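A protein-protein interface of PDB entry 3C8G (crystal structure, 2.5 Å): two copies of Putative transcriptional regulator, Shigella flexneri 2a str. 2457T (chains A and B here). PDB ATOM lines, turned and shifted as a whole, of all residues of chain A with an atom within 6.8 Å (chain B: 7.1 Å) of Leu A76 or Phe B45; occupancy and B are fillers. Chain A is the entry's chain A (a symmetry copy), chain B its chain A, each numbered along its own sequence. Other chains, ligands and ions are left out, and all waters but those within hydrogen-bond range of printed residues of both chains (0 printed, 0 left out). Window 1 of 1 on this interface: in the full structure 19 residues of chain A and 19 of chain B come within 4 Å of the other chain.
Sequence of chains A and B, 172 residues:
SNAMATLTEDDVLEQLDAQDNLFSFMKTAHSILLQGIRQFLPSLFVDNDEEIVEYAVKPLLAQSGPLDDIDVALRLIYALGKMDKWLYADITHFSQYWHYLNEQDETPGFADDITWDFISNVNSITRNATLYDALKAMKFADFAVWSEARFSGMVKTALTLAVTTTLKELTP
N of Val B46 lies within hydrogen-bond range of O of Ala A79, 2.8 Å away.
The backbone carbonyl oxygen of Ile B52 sits at hydrogen-bond distance from the backbone NH of Val B57, at 2.9 Å.
Leu B76 touches Phe A45 (CD2 to CE1, 3.6 Å). CD1 of Phe A45 touches CD2 of Leu B80 (3.6 Å). Leu B60 touches Arg A75. Tyr A78 touches Ile B52. CB of Ala B56 touches CD2 of Tyr A78, at 3.99 Å. Phe B45 touches Ala A79. Ala A79 touches Ile B52. Val B57 touches Ala A79. Leu A80 touches Leu B44 (CD2 to O, 3.4 Å). CD2 of Leu A80 touches CD1 of Phe B45 (3.6 Å).
Leu A76 touches just these residues of chain B: Phe B45 and Leu B60. Of chain A, only Leu A76, Ala A79 and Leu A80 come within 4 Å of Phe B45. Of the printed residues of chain A, Val B46 touches Ala A79 and Gly A81. Of the printed residues of chain A, Leu B76 touches Phe A45 (3.6 Å). The nearest residue of chain B that does not touch Leu A76 is Leu B76 (4.05 Å). The nearest printed residue of chain B that does not touch Leu A80 is Val B46 (4.4 Å).
Hydrophobic or aromatic side chains of chain B that line the printed part of chain A: Phe B45, Val B46, Ile B52, Ala B56, Val B57, Leu B60, Leu B76 and Leu B80. Printed residues of chain A that touch a printed residue of chain B: Leu A44, Phe A45, Val A72, Arg A75, Leu A76, Tyr A78, Ala A79, Leu A80 and Gly A81. Hydrophobic or aromatic side chains of chain A within 4 Å of the printed part of chain B: Phe A45, Leu A76, Tyr A78, Ala A79 and Leu A80. Along chain A the printed residues that touch a printed residue of chain B span positions 44 to 81.
Leu A44 touches Leu B80, and with the chains exchanged Leu A80 touches Leu B44. Phe A45 touches Leu B76, and with the chains exchanged Leu A76 touches Phe B45. Phe A45 touches Leu B80, and with the chains exchanged Leu A80 touches Phe B45. Leu B80 touches its own counterpart, Leu A80. Of the 19 pairs that touch across the chains among the printed residues, 7 have their exchanged pair printed and touching as well.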
ATOM      1  N   LEU A  41     -36.643 -26.001   2.674  1.00  0.00           N
ATOM      2  CA  LEU A  41     -36.413 -25.380   1.377  1.00  0.00           C
ATOM      3  C   LEU A  41     -37.111 -24.046   1.182  1.00  0.00           C
ATOM      4  O   LEU A  41     -36.474 -23.096   0.761  1.00  0.00           O
ATOM      5  CB  LEU A  41     -36.734 -26.353   0.260  1.00  0.00           C
ATOM      6  CG  LEU A  41     -35.527 -27.041  -0.382  1.00  0.00           C
ATOM      7  CD1 LEU A  41     -34.317 -27.033   0.506  1.00  0.00           C
ATOM      8  CD2 LEU A  41     -35.886 -28.436  -0.846  1.00  0.00           C
ATOM      9  N   LEU A  44     -35.186 -20.768   1.948  1.00  0.00           N
ATOM     10  CA  LEU A  44     -34.247 -20.264   0.949  1.00  0.00           C
ATOM     11  C   LEU A  44     -34.771 -19.133   0.062  1.00  0.00           C
ATOM     12  O   LEU A  44     -34.005 -18.427  -0.569  1.00  0.00           O
ATOM     13  CB  LEU A  44     -33.868 -21.412   0.003  1.00  0.00           C
ATOM     14  CG  LEU A  44     -32.653 -22.307   0.293  1.00  0.00           C
ATOM     15  CD1 LEU A  44     -32.097 -22.185   1.690  1.00  0.00           C
ATOM     16  CD2 LEU A  44     -32.957 -23.773  -0.134  1.00  0.00           C
ATOM     17  N   PHE A  45     -36.078 -18.997  -0.028  1.00  0.00           N
ATOM     18  CA  PHE A  45     -36.657 -18.221  -1.117  1.00  0.00           C
ATOM     19  C   PHE A  45     -37.484 -17.036  -0.639  1.00  0.00           C
ATOM     20  O   PHE A  45     -37.737 -16.891   0.541  1.00  0.00           O
ATOM     21  CB  PHE A  45     -37.511 -19.108  -2.066  1.00  0.00           C
ATOM     22  CG  PHE A  45     -36.777 -20.269  -2.627  1.00  0.00           C
ATOM     23  CD1 PHE A  45     -35.649 -20.078  -3.421  1.00  0.00           C
ATOM     24  CD2 PHE A  45     -37.201 -21.580  -2.360  1.00  0.00           C
ATOM     25  CE1 PHE A  45     -34.941 -21.165  -3.935  1.00  0.00           C
ATOM     26  CE2 PHE A  45     -36.510 -22.686  -2.894  1.00  0.00           C
ATOM     27  CZ  PHE A  45     -35.382 -22.478  -3.668  1.00  0.00           C
ATOM     28  N   LEU A  67     -36.149 -30.368  -6.998  1.00  0.00           N
ATOM     29  CA  LEU A  67     -35.516 -30.369  -5.699  1.00  0.00           C
ATOM     30  C   LEU A  67     -35.900 -31.561  -4.841  1.00  0.00           C
ATOM     31  O   LEU A  67     -35.530 -31.628  -3.683  1.00  0.00           O
ATOM     32  CB  LEU A  67     -35.749 -29.057  -4.953  1.00  0.00           C
ATOM     33  CG  LEU A  67     -35.093 -27.840  -5.571  1.00  0.00           C
ATOM     34  CD1 LEU A  67     -35.546 -26.671  -4.770  1.00  0.00           C
ATOM     35  CD2 LEU A  67     -33.576 -27.946  -5.564  1.00  0.00           C
ATOM     36  N   ASP A  71     -29.914 -35.100  -2.465  1.00  0.00           N
ATOM     37  CA  ASP A  71     -28.576 -34.709  -2.854  1.00  0.00           C
ATOM     38  C   ASP A  71     -28.543 -33.396  -3.655  1.00  0.00           C
ATOM     39  O   ASP A  71     -27.711 -32.542  -3.351  1.00  0.00           O
ATOM     40  CB  ASP A  71     -27.862 -35.856  -3.558  1.00  0.00           C
ATOM     41  CG  ASP A  71     -27.708 -37.099  -2.651  1.00  0.00           C
ATOM     42  OD1 ASP A  71     -27.663 -36.952  -1.426  1.00  0.00           O
ATOM     43  OD2 ASP A  71     -27.617 -38.233  -3.164  1.00  0.00           O
ATOM     44  N   VAL A  72     -29.431 -33.192  -4.630  1.00  0.00           N
ATOM     45  CA  VAL A  72     -29.553 -31.836  -5.166  1.00  0.00           C
ATOM     46  C   VAL A  72     -30.048 -30.803  -4.111  1.00  0.00           C
ATOM     47  O   VAL A  72     -29.504 -29.696  -4.052  1.00  0.00           O
ATOM     48  CB  VAL A  72     -30.280 -31.718  -6.548  1.00  0.00           C
ATOM     49  CG1 VAL A  72     -30.349 -33.054  -7.273  1.00  0.00           C
ATOM     50  CG2 VAL A  72     -31.610 -31.161  -6.380  1.00  0.00           C
ATOM     51  N   ALA A  73     -30.969 -31.151  -3.213  1.00  0.00           N
ATOM     52  CA  ALA A  73     -31.447 -30.141  -2.256  1.00  0.00           C
ATOM     53  C   ALA A  73     -30.356 -29.688  -1.262  1.00  0.00           C
ATOM     54  O   ALA A  73     -30.232 -28.499  -0.930  1.00  0.00           O
ATOM     55  CB  ALA A  73     -32.700 -30.607  -1.543  1.00  0.00           C
ATOM     56  N   LEU A  74     -29.560 -30.642  -0.798  1.00  0.00           N
ATOM     57  CA  LEU A  74     -28.463 -30.357   0.112  1.00  0.00           C
ATOM     58  C   LEU A  74     -27.458 -29.467  -0.508  1.00  0.00           C
ATOM     59  O   LEU A  74     -27.047 -28.478   0.082  1.00  0.00           O
ATOM     60  CB  LEU A  74     -27.741 -31.647   0.483  1.00  0.00           C
ATOM     61  CG  LEU A  74     -28.038 -32.223   1.845  1.00  0.00           C
ATOM     62  CD1 LEU A  74     -27.404 -33.589   1.852  1.00  0.00           C
ATOM     63  CD2 LEU A  74     -27.503 -31.326   2.995  1.00  0.00           C
ATOM     64  N   ARG A  75     -27.033 -29.862  -1.691  1.00  0.00           N
ATOM     65  CA  ARG A  75     -26.087 -29.067  -2.467  1.00  0.00           C
ATOM     66  C   ARG A  75     -26.537 -27.604  -2.648  1.00  0.00           C
ATOM     67  O   ARG A  75     -25.710 -26.715  -2.517  1.00  0.00           O
ATOM     68  CB  ARG A  75     -25.735 -29.744  -3.801  1.00  0.00           C
ATOM     69  CG  ARG A  75     -24.921 -30.995  -3.560  1.00  0.00           C
ATOM     70  CD  ARG A  75     -24.255 -31.502  -4.795  1.00  0.00           C
ATOM     71  NE  ARG A  75     -25.051 -32.376  -5.641  1.00  0.00           N
ATOM     72  CZ  ARG A  75     -24.883 -33.699  -5.765  1.00  0.00           C
ATOM     73  NH1 ARG A  75     -23.962 -34.345  -5.046  1.00  0.00           N
ATOM     74  NH2 ARG A  75     -25.665 -34.376  -6.608  1.00  0.00           N
ATOM     75  N   LEU A  76     -27.830 -27.380  -2.905  1.00  0.00           N
ATOM     76  CA  LEU A  76     -28.390 -26.042  -3.025  1.00  0.00           C
ATOM     77  C   LEU A  76     -28.233 -25.290  -1.678  1.00  0.00           C
ATOM     78  O   LEU A  76     -27.686 -24.175  -1.640  1.00  0.00           O
ATOM     79  CB  LEU A  76     -29.850 -26.121  -3.476  1.00  0.00           C
ATOM     80  CG  LEU A  76     -30.661 -25.096  -4.326  1.00  0.00           C
ATOM     81  CD1 LEU A  76     -31.863 -24.538  -3.604  1.00  0.00           C
ATOM     82  CD2 LEU A  76     -29.872 -23.970  -5.013  1.00  0.00           C
ATOM     83  N   ILE A  77     -28.657 -25.893  -0.567  1.00  0.00           N
ATOM     84  CA  ILE A  77     -28.618 -25.185   0.720  1.00  0.00           C
ATOM     85  C   ILE A  77     -27.170 -24.827   1.041  1.00  0.00           C
ATOM     86  O   ILE A  77     -26.852 -23.715   1.499  1.00  0.00           O
ATOM     87  CB  ILE A  77     -29.197 -26.009   1.858  1.00  0.00           C
ATOM     88  CG1 ILE A  77     -30.673 -26.348   1.605  1.00  0.00           C
ATOM     89  CG2 ILE A  77     -28.971 -25.283   3.232  1.00  0.00           C
ATOM     90  CD1 ILE A  77     -31.281 -27.355   2.640  1.00  0.00           C
ATOM     91  N   TYR A  78     -26.287 -25.782   0.803  1.00  0.00           N
ATOM     92  CA  TYR A  78     -24.881 -25.584   1.046  1.00  0.00           C
ATOM     93  C   TYR A  78     -24.339 -24.481   0.136  1.00  0.00           C
ATOM     94  O   TYR A  78     -23.654 -23.581   0.595  1.00  0.00           O
ATOM     95  CB  TYR A  78     -24.147 -26.903   0.814  1.00  0.00           C
ATOM     96  CG  TYR A  78     -22.808 -26.994   1.480  1.00  0.00           C
ATOM     97  CD1 TYR A  78     -22.581 -26.393   2.702  1.00  0.00           C
ATOM     98  CD2 TYR A  78     -21.770 -27.693   0.878  1.00  0.00           C
ATOM     99  CE1 TYR A  78     -21.338 -26.465   3.316  1.00  0.00           C
ATOM    100  CE2 TYR A  78     -20.521 -27.781   1.476  1.00  0.00           C
ATOM    101  CZ  TYR A  78     -20.308 -27.167   2.692  1.00  0.00           C
ATOM    102  OH  TYR A  78     -19.069 -27.263   3.290  1.00  0.00           O
ATOM    103  N   ALA A  79     -24.681 -24.545  -1.145  1.00  0.00           N
ATOM    104  CA  ALA A  79     -24.195 -23.562  -2.135  1.00  0.00           C
ATOM    105  C   ALA A  79     -24.723 -22.134  -1.903  1.00  0.00           C
ATOM    106  O   ALA A  79     -24.142 -21.155  -2.396  1.00  0.00           O
ATOM    107  CB  ALA A  79     -24.492 -24.030  -3.558  1.00  0.00           C
ATOM    108  N   LEU A  80     -25.817 -22.007  -1.157  1.00  0.00           N
ATOM    109  CA  LEU A  80     -26.353 -20.687  -0.870  1.00  0.00           C
ATOM    110  C   LEU A  80     -25.753 -20.117   0.421  1.00  0.00           C
ATOM    111  O   LEU A  80     -26.072 -19.006   0.836  1.00  0.00           O
ATOM    112  CB  LEU A  80     -27.895 -20.682  -0.847  1.00  0.00           C
ATOM    113  CG  LEU A  80     -28.622 -20.941  -2.173  1.00  0.00           C
ATOM    114  CD1 LEU A  80     -30.087 -21.247  -1.955  1.00  0.00           C
ATOM    115  CD2 LEU A  80     -28.472 -19.805  -3.172  1.00  0.00           C
ATOM    116  N   GLY A  81     -24.864 -20.880   1.040  1.00  0.00           N
ATOM    117  CA  GLY A  81     -24.245 -20.500   2.322  1.00  0.00           C
ATOM    118  C   GLY A  81     -25.198 -20.637   3.497  1.00  0.00           C
ATOM    119  O   GLY A  81     -25.053 -19.928   4.495  1.00  0.00           O
ATOM    120  N   MLY A  82     -26.161 -21.558   3.407  1.00  0.00           N
ATOM    121  CA  MLY A  82     -27.173 -21.701   4.461  1.00  0.00           C
ATOM    122  CB  MLY A  82     -28.587 -21.445   3.891  1.00  0.00           C
ATOM    123  CG  MLY A  82     -28.745 -20.078   3.187  1.00  0.00           C
ATOM    124  CD  MLY A  82     -29.295 -18.927   4.056  1.00  0.00           C
ATOM    125  CE  MLY A  82     -29.385 -17.554   3.342  1.00  0.00           C
ATOM    126  NZ  MLY A  82     -30.692 -17.377   2.664  1.00  0.00           N
ATOM    127  CH1 MLY A  82     -30.771 -17.242   1.217  1.00  0.00           C
ATOM    128  CH2 MLY A  82     -31.955 -17.342   3.400  1.00  0.00           C
ATOM    129  C   MLY A  82     -26.997 -22.942   5.342  1.00  0.00           C
ATOM    130  O   MLY A  82     -27.863 -23.266   6.160  1.00  0.00           O
ATOM    131  N   TYR A  88     -23.565 -30.427   6.728  1.00  0.00           N
ATOM    132  CA  TYR A  88     -23.588 -30.949   5.379  1.00  0.00           C
ATOM    133  C   TYR A  88     -22.908 -32.337   5.340  1.00  0.00           C
ATOM    134  O   TYR A  88     -23.435 -33.283   4.716  1.00  0.00           O
ATOM    135  CB  TYR A  88     -22.961 -29.959   4.402  1.00  0.00           C
ATOM    136  CG  TYR A  88     -22.757 -30.483   2.988  1.00  0.00           C
ATOM    137  CD1 TYR A  88     -21.541 -31.010   2.607  1.00  0.00           C
ATOM    138  CD2 TYR A  88     -23.778 -30.449   2.049  1.00  0.00           C
ATOM    139  CE1 TYR A  88     -21.317 -31.497   1.339  1.00  0.00           C
ATOM    140  CE2 TYR A  88     -23.579 -30.937   0.738  1.00  0.00           C
ATOM    141  CZ  TYR A  88     -22.330 -31.455   0.399  1.00  0.00           C
ATOM    142  OH  TYR A  88     -22.054 -31.931  -0.866  1.00  0.00           O
ATOM    143  N   PHE B  40     -24.926 -16.795 -15.438  1.00  0.00           N
ATOM    144  CA  PHE B  40     -25.330 -15.957 -14.313  1.00  0.00           C
ATOM    145  C   PHE B  40     -25.440 -16.798 -13.040  1.00  0.00           C
ATOM    146  O   PHE B  40     -25.293 -16.280 -11.939  1.00  0.00           O
ATOM    147  CB  PHE B  40     -26.693 -15.343 -14.611  1.00  0.00           C
ATOM    148  CG  PHE B  40     -27.256 -14.537 -13.490  1.00  0.00           C
ATOM    149  CD1 PHE B  40     -28.027 -15.142 -12.507  1.00  0.00           C
ATOM    150  CD2 PHE B  40     -27.019 -13.173 -13.418  1.00  0.00           C
ATOM    151  CE1 PHE B  40     -28.538 -14.401 -11.443  1.00  0.00           C
ATOM    152  CE2 PHE B  40     -27.539 -12.397 -12.376  1.00  0.00           C
ATOM    153  CZ  PHE B  40     -28.297 -13.001 -11.394  1.00  0.00           C
ATOM    154  N   LEU B  41     -25.682 -18.092 -13.204  1.00  0.00           N
ATOM    155  CA  LEU B  41     -25.978 -18.970 -12.080  1.00  0.00           C
ATOM    156  C   LEU B  41     -24.935 -18.958 -10.976  1.00  0.00           C
ATOM    157  O   LEU B  41     -25.294 -18.818  -9.820  1.00  0.00           O
ATOM    158  CB  LEU B  41     -26.266 -20.376 -12.568  1.00  0.00           C
ATOM    159  CG  LEU B  41     -27.747 -20.755 -12.647  1.00  0.00           C
ATOM    160  CD1 LEU B  41     -28.648 -19.557 -12.721  1.00  0.00           C
ATOM    161  CD2 LEU B  41     -27.994 -21.727 -13.781  1.00  0.00           C
ATOM    162  N   PRO B  42     -23.637 -19.014 -11.320  1.00  0.00           N
ATOM    163  CA  PRO B  42     -22.657 -18.910 -10.201  1.00  0.00           C
ATOM    164  C   PRO B  42     -22.785 -17.658  -9.284  1.00  0.00           C
ATOM    165  O   PRO B  42     -22.351 -17.718  -8.145  1.00  0.00           O
ATOM    166  CB  PRO B  42     -21.298 -18.894 -10.904  1.00  0.00           C
ATOM    167  CG  PRO B  42     -21.543 -19.452 -12.272  1.00  0.00           C
ATOM    168  CD  PRO B  42     -22.986 -19.150 -12.639  1.00  0.00           C
ATOM    169  N   SER B  43     -23.373 -16.546  -9.723  1.00  0.00           N
ATOM    170  CA  SER B  43     -23.497 -15.401  -8.825  1.00  0.00           C
ATOM    171  C   SER B  43     -24.566 -15.608  -7.755  1.00  0.00           C
ATOM    172  O   SER B  43     -24.605 -14.899  -6.747  1.00  0.00           O
ATOM    173  CB  SER B  43     -23.693 -14.082  -9.593  1.00  0.00           C
ATOM    174  OG  SER B  43     -24.861 -14.078 -10.404  1.00  0.00           O
ATOM    175  N   LEU B  44     -25.416 -16.599  -7.938  1.00  0.00           N
ATOM    176  CA  LEU B  44     -26.332 -17.010  -6.876  1.00  0.00           C
ATOM    177  C   LEU B  44     -25.673 -17.617  -5.636  1.00  0.00           C
ATOM    178  O   LEU B  44     -26.280 -17.697  -4.582  1.00  0.00           O
ATOM    179  CB  LEU B  44     -27.279 -18.083  -7.429  1.00  0.00           C
ATOM    180  CG  LEU B  44     -28.625 -17.698  -8.064  1.00  0.00           C
ATOM    181  CD1 LEU B  44     -28.775 -16.233  -8.389  1.00  0.00           C
ATOM    182  CD2 LEU B  44     -28.938 -18.641  -9.262  1.00  0.00           C
ATOM    183  N   PHE B  45     -24.454 -18.095  -5.775  1.00  0.00           N
ATOM    184  CA  PHE B  45     -23.911 -19.012  -4.782  1.00  0.00           C
ATOM    185  C   PHE B  45     -22.648 -18.493  -4.111  1.00  0.00           C
ATOM    186  O   PHE B  45     -22.099 -17.485  -4.513  1.00  0.00           O
ATOM    187  CB  PHE B  45     -23.645 -20.420  -5.383  1.00  0.00           C
ATOM    188  CG  PHE B  45     -24.835 -21.037  -6.021  1.00  0.00           C
ATOM    189  CD1 PHE B  45     -25.981 -21.301  -5.277  1.00  0.00           C
ATOM    190  CD2 PHE B  45     -24.827 -21.356  -7.388  1.00  0.00           C
ATOM    191  CE1 PHE B  45     -27.111 -21.861  -5.875  1.00  0.00           C
ATOM    192  CE2 PHE B  45     -25.953 -21.944  -7.998  1.00  0.00           C
ATOM    193  CZ  PHE B  45     -27.090 -22.186  -7.247  1.00  0.00           C
ATOM    194  N   VAL B  46     -22.218 -19.203  -3.060  1.00  0.00           N
ATOM    195  CA  VAL B  46     -20.908 -19.028  -2.491  1.00  0.00           C
ATOM    196  C   VAL B  46     -19.792 -19.088  -3.535  1.00  0.00           C
ATOM    197  O   VAL B  46     -19.828 -19.844  -4.507  1.00  0.00           O
ATOM    198  CB  VAL B  46     -20.646 -20.009  -1.384  1.00  0.00           C
ATOM    199  CG1 VAL B  46     -19.175 -20.030  -1.063  1.00  0.00           C
ATOM    200  CG2 VAL B  46     -21.444 -19.602  -0.162  1.00  0.00           C
ATOM    201  N   ASP B  47     -18.781 -18.284  -3.251  1.00  0.00           N
ATOM    202  CA  ASP B  47     -17.830 -17.796  -4.179  1.00  0.00           C
ATOM    203  C   ASP B  47     -16.448 -18.158  -3.690  1.00  0.00           C
ATOM    204  O   ASP B  47     -15.598 -18.603  -4.451  1.00  0.00           O
ATOM    205  CB  ASP B  47     -17.941 -16.281  -4.090  1.00  0.00           C
ATOM    206  CG  ASP B  47     -17.601 -15.627  -5.342  1.00  0.00           C
ATOM    207  OD1 ASP B  47     -17.282 -16.385  -6.275  1.00  0.00           O
ATOM    208  OD2 ASP B  47     -17.654 -14.372  -5.412  1.00  0.00           O
ATOM    209  N   ASN B  48     -16.248 -17.981  -2.394  1.00  0.00           N
ATOM    210  CA  ASN B  48     -14.926 -17.863  -1.827  1.00  0.00           C
ATOM    211  C   ASN B  48     -14.467 -19.064  -0.972  1.00  0.00           C
ATOM    212  O   ASN B  48     -13.419 -19.000  -0.344  1.00  0.00           O
ATOM    213  CB  ASN B  48     -14.887 -16.563  -1.008  1.00  0.00           C
ATOM    214  CG  ASN B  48     -15.943 -16.541   0.107  1.00  0.00           C
ATOM    215  OD1 ASN B  48     -16.649 -17.530   0.324  1.00  0.00           O
ATOM    216  ND2 ASN B  48     -16.054 -15.419   0.807  1.00  0.00           N
ATOM    217  N   ILE B  52     -17.438 -25.775  -0.989  1.00  0.00           N
ATOM    218  CA  ILE B  52     -18.747 -25.507  -1.510  1.00  0.00           C
ATOM    219  C   ILE B  52     -18.738 -25.525  -3.048  1.00  0.00           C
ATOM    220  O   ILE B  52     -19.612 -26.140  -3.678  1.00  0.00           O
ATOM    221  CB  ILE B  52     -19.312 -24.210  -0.907  1.00  0.00           C
ATOM    222  CG1 ILE B  52     -19.341 -24.341   0.620  1.00  0.00           C
ATOM    223  CG2 ILE B  52     -20.684 -23.952  -1.444  1.00  0.00           C
ATOM    224  CD1 ILE B  52     -19.978 -23.200   1.400  1.00  0.00           C
ATOM    225  N   ALA B  56     -20.578 -28.788  -4.176  1.00  0.00           N
ATOM    226  CA  ALA B  56     -21.984 -28.376  -4.265  1.00  0.00           C
ATOM    227  C   ALA B  56     -22.269 -27.626  -5.553  1.00  0.00           C
ATOM    228  O   ALA B  56     -23.120 -28.066  -6.325  1.00  0.00           O
ATOM    229  CB  ALA B  56     -22.430 -27.566  -3.054  1.00  0.00           C
ATOM    230  N   VAL B  57     -21.562 -26.515  -5.794  1.00  0.00           N
ATOM    231  CA  VAL B  57     -21.859 -25.663  -6.948  1.00  0.00           C
ATOM    232  C   VAL B  57     -21.673 -26.389  -8.282  1.00  0.00           C
ATOM    233  O   VAL B  57     -22.582 -26.407  -9.100  1.00  0.00           O
ATOM    234  CB  VAL B  57     -21.075 -24.309  -6.932  1.00  0.00           C
ATOM    235  CG1 VAL B  57     -21.315 -23.537  -8.201  1.00  0.00           C
ATOM    236  CG2 VAL B  57     -21.472 -23.463  -5.758  1.00  0.00           C
ATOM    237  N   LEU B  60     -24.231 -28.870  -9.219  1.00  0.00           N
ATOM    238  CA  LEU B  60     -25.477 -28.159  -9.369  1.00  0.00           C
ATOM    239  C   LEU B  60     -25.537 -27.521 -10.784  1.00  0.00           C
ATOM    240  O   LEU B  60     -26.615 -27.373 -11.358  1.00  0.00           O
ATOM    241  CB  LEU B  60     -25.536 -27.101  -8.279  1.00  0.00           C
ATOM    242  CG  LEU B  60     -26.655 -26.914  -7.263  1.00  0.00           C
ATOM    243  CD1 LEU B  60     -27.464 -28.185  -6.992  1.00  0.00           C
ATOM    244  CD2 LEU B  60     -26.017 -26.372  -5.978  1.00  0.00           C
ATOM    245  N   LEU B  61     -24.381 -27.178 -11.346  1.00  0.00           N
ATOM    246  CA  LEU B  61     -24.312 -26.505 -12.643  1.00  0.00           C
ATOM    247  C   LEU B  61     -23.720 -27.335 -13.778  1.00  0.00           C
ATOM    248  O   LEU B  61     -23.448 -26.788 -14.839  1.00  0.00           O
ATOM    249  CB  LEU B  61     -23.481 -25.232 -12.534  1.00  0.00           C
ATOM    250  CG  LEU B  61     -23.962 -24.231 -11.504  1.00  0.00           C
ATOM    251  CD1 LEU B  61     -23.133 -22.989 -11.612  1.00  0.00           C
ATOM    252  CD2 LEU B  61     -25.439 -23.919 -11.674  1.00  0.00           C
ATOM    253  N   LEU B  67     -29.802 -27.884 -13.088  1.00  0.00           N
ATOM    254  CA  LEU B  67     -30.086 -26.518 -13.465  1.00  0.00           C
ATOM    255  C   LEU B  67     -29.942 -26.261 -14.955  1.00  0.00           C
ATOM    256  O   LEU B  67     -30.039 -25.130 -15.394  1.00  0.00           O
ATOM    257  CB  LEU B  67     -29.262 -25.521 -12.653  1.00  0.00           C
ATOM    258  CG  LEU B  67     -29.592 -25.466 -11.176  1.00  0.00           C
ATOM    259  CD1 LEU B  67     -28.602 -24.539 -10.563  1.00  0.00           C
ATOM    260  CD2 LEU B  67     -31.012 -24.982 -10.929  1.00  0.00           C
ATOM    261  N   LEU B  76     -35.467 -20.509 -10.187  1.00  0.00           N
ATOM    262  CA  LEU B  76     -34.532 -20.383  -9.079  1.00  0.00           C
ATOM    263  C   LEU B  76     -34.117 -18.898  -8.915  1.00  0.00           C
ATOM    264  O   LEU B  76     -34.232 -18.329  -7.817  1.00  0.00           O
ATOM    265  CB  LEU B  76     -33.328 -21.300  -9.299  1.00  0.00           C
ATOM    266  CG  LEU B  76     -32.435 -22.004  -8.233  1.00  0.00           C
ATOM    267  CD1 LEU B  76     -30.984 -21.593  -8.302  1.00  0.00           C
ATOM    268  CD2 LEU B  76     -32.933 -21.994  -6.779  1.00  0.00           C
ATOM    269  N   LEU B  80     -35.101 -16.589  -5.663  1.00  0.00           N
ATOM    270  CA  LEU B  80     -34.101 -16.099  -4.728  1.00  0.00           C
ATOM    271  C   LEU B  80     -34.163 -14.571  -4.603  1.00  0.00           C
ATOM    272  O   LEU B  80     -33.404 -13.961  -3.856  1.00  0.00           O
ATOM    273  CB  LEU B  80     -32.685 -16.596  -5.083  1.00  0.00           C
ATOM    274  CG  LEU B  80     -32.409 -18.099  -4.946  1.00  0.00           C
ATOM    275  CD1 LEU B  80     -31.124 -18.495  -5.639  1.00  0.00           C
ATOM    276  CD2 LEU B  80     -32.391 -18.577  -3.503  1.00  0.00           C
ATOM    277  N   MLY B  82     -33.598 -12.513  -7.173  1.00  0.00           N
ATOM    278  CA  MLY B  82     -32.481 -11.963  -7.952  1.00  0.00           C
ATOM    279  CB  MLY B  82     -31.233 -12.865  -7.818  1.00  0.00           C
ATOM    280  CG  MLY B  82     -30.788 -13.112  -6.358  1.00  0.00           C
ATOM    281  CD  MLY B  82     -29.701 -12.164  -5.810  1.00  0.00           C
ATOM    282  CE  MLY B  82     -29.318 -12.395  -4.326  1.00  0.00           C
ATOM    283  NZ  MLY B  82     -28.218 -13.382  -4.194  1.00  0.00           N
ATOM    284  CH1 MLY B  82     -28.429 -14.650  -3.512  1.00  0.00           C
ATOM    285  CH2 MLY B  82     -26.885 -13.143  -4.745  1.00  0.00           C
ATOM    286  C   MLY B  82     -32.860 -11.513  -9.367  1.00  0.00           C
ATOM    287  O   MLY B  82     -31.992 -11.181 -10.178  1.00  0.00           O
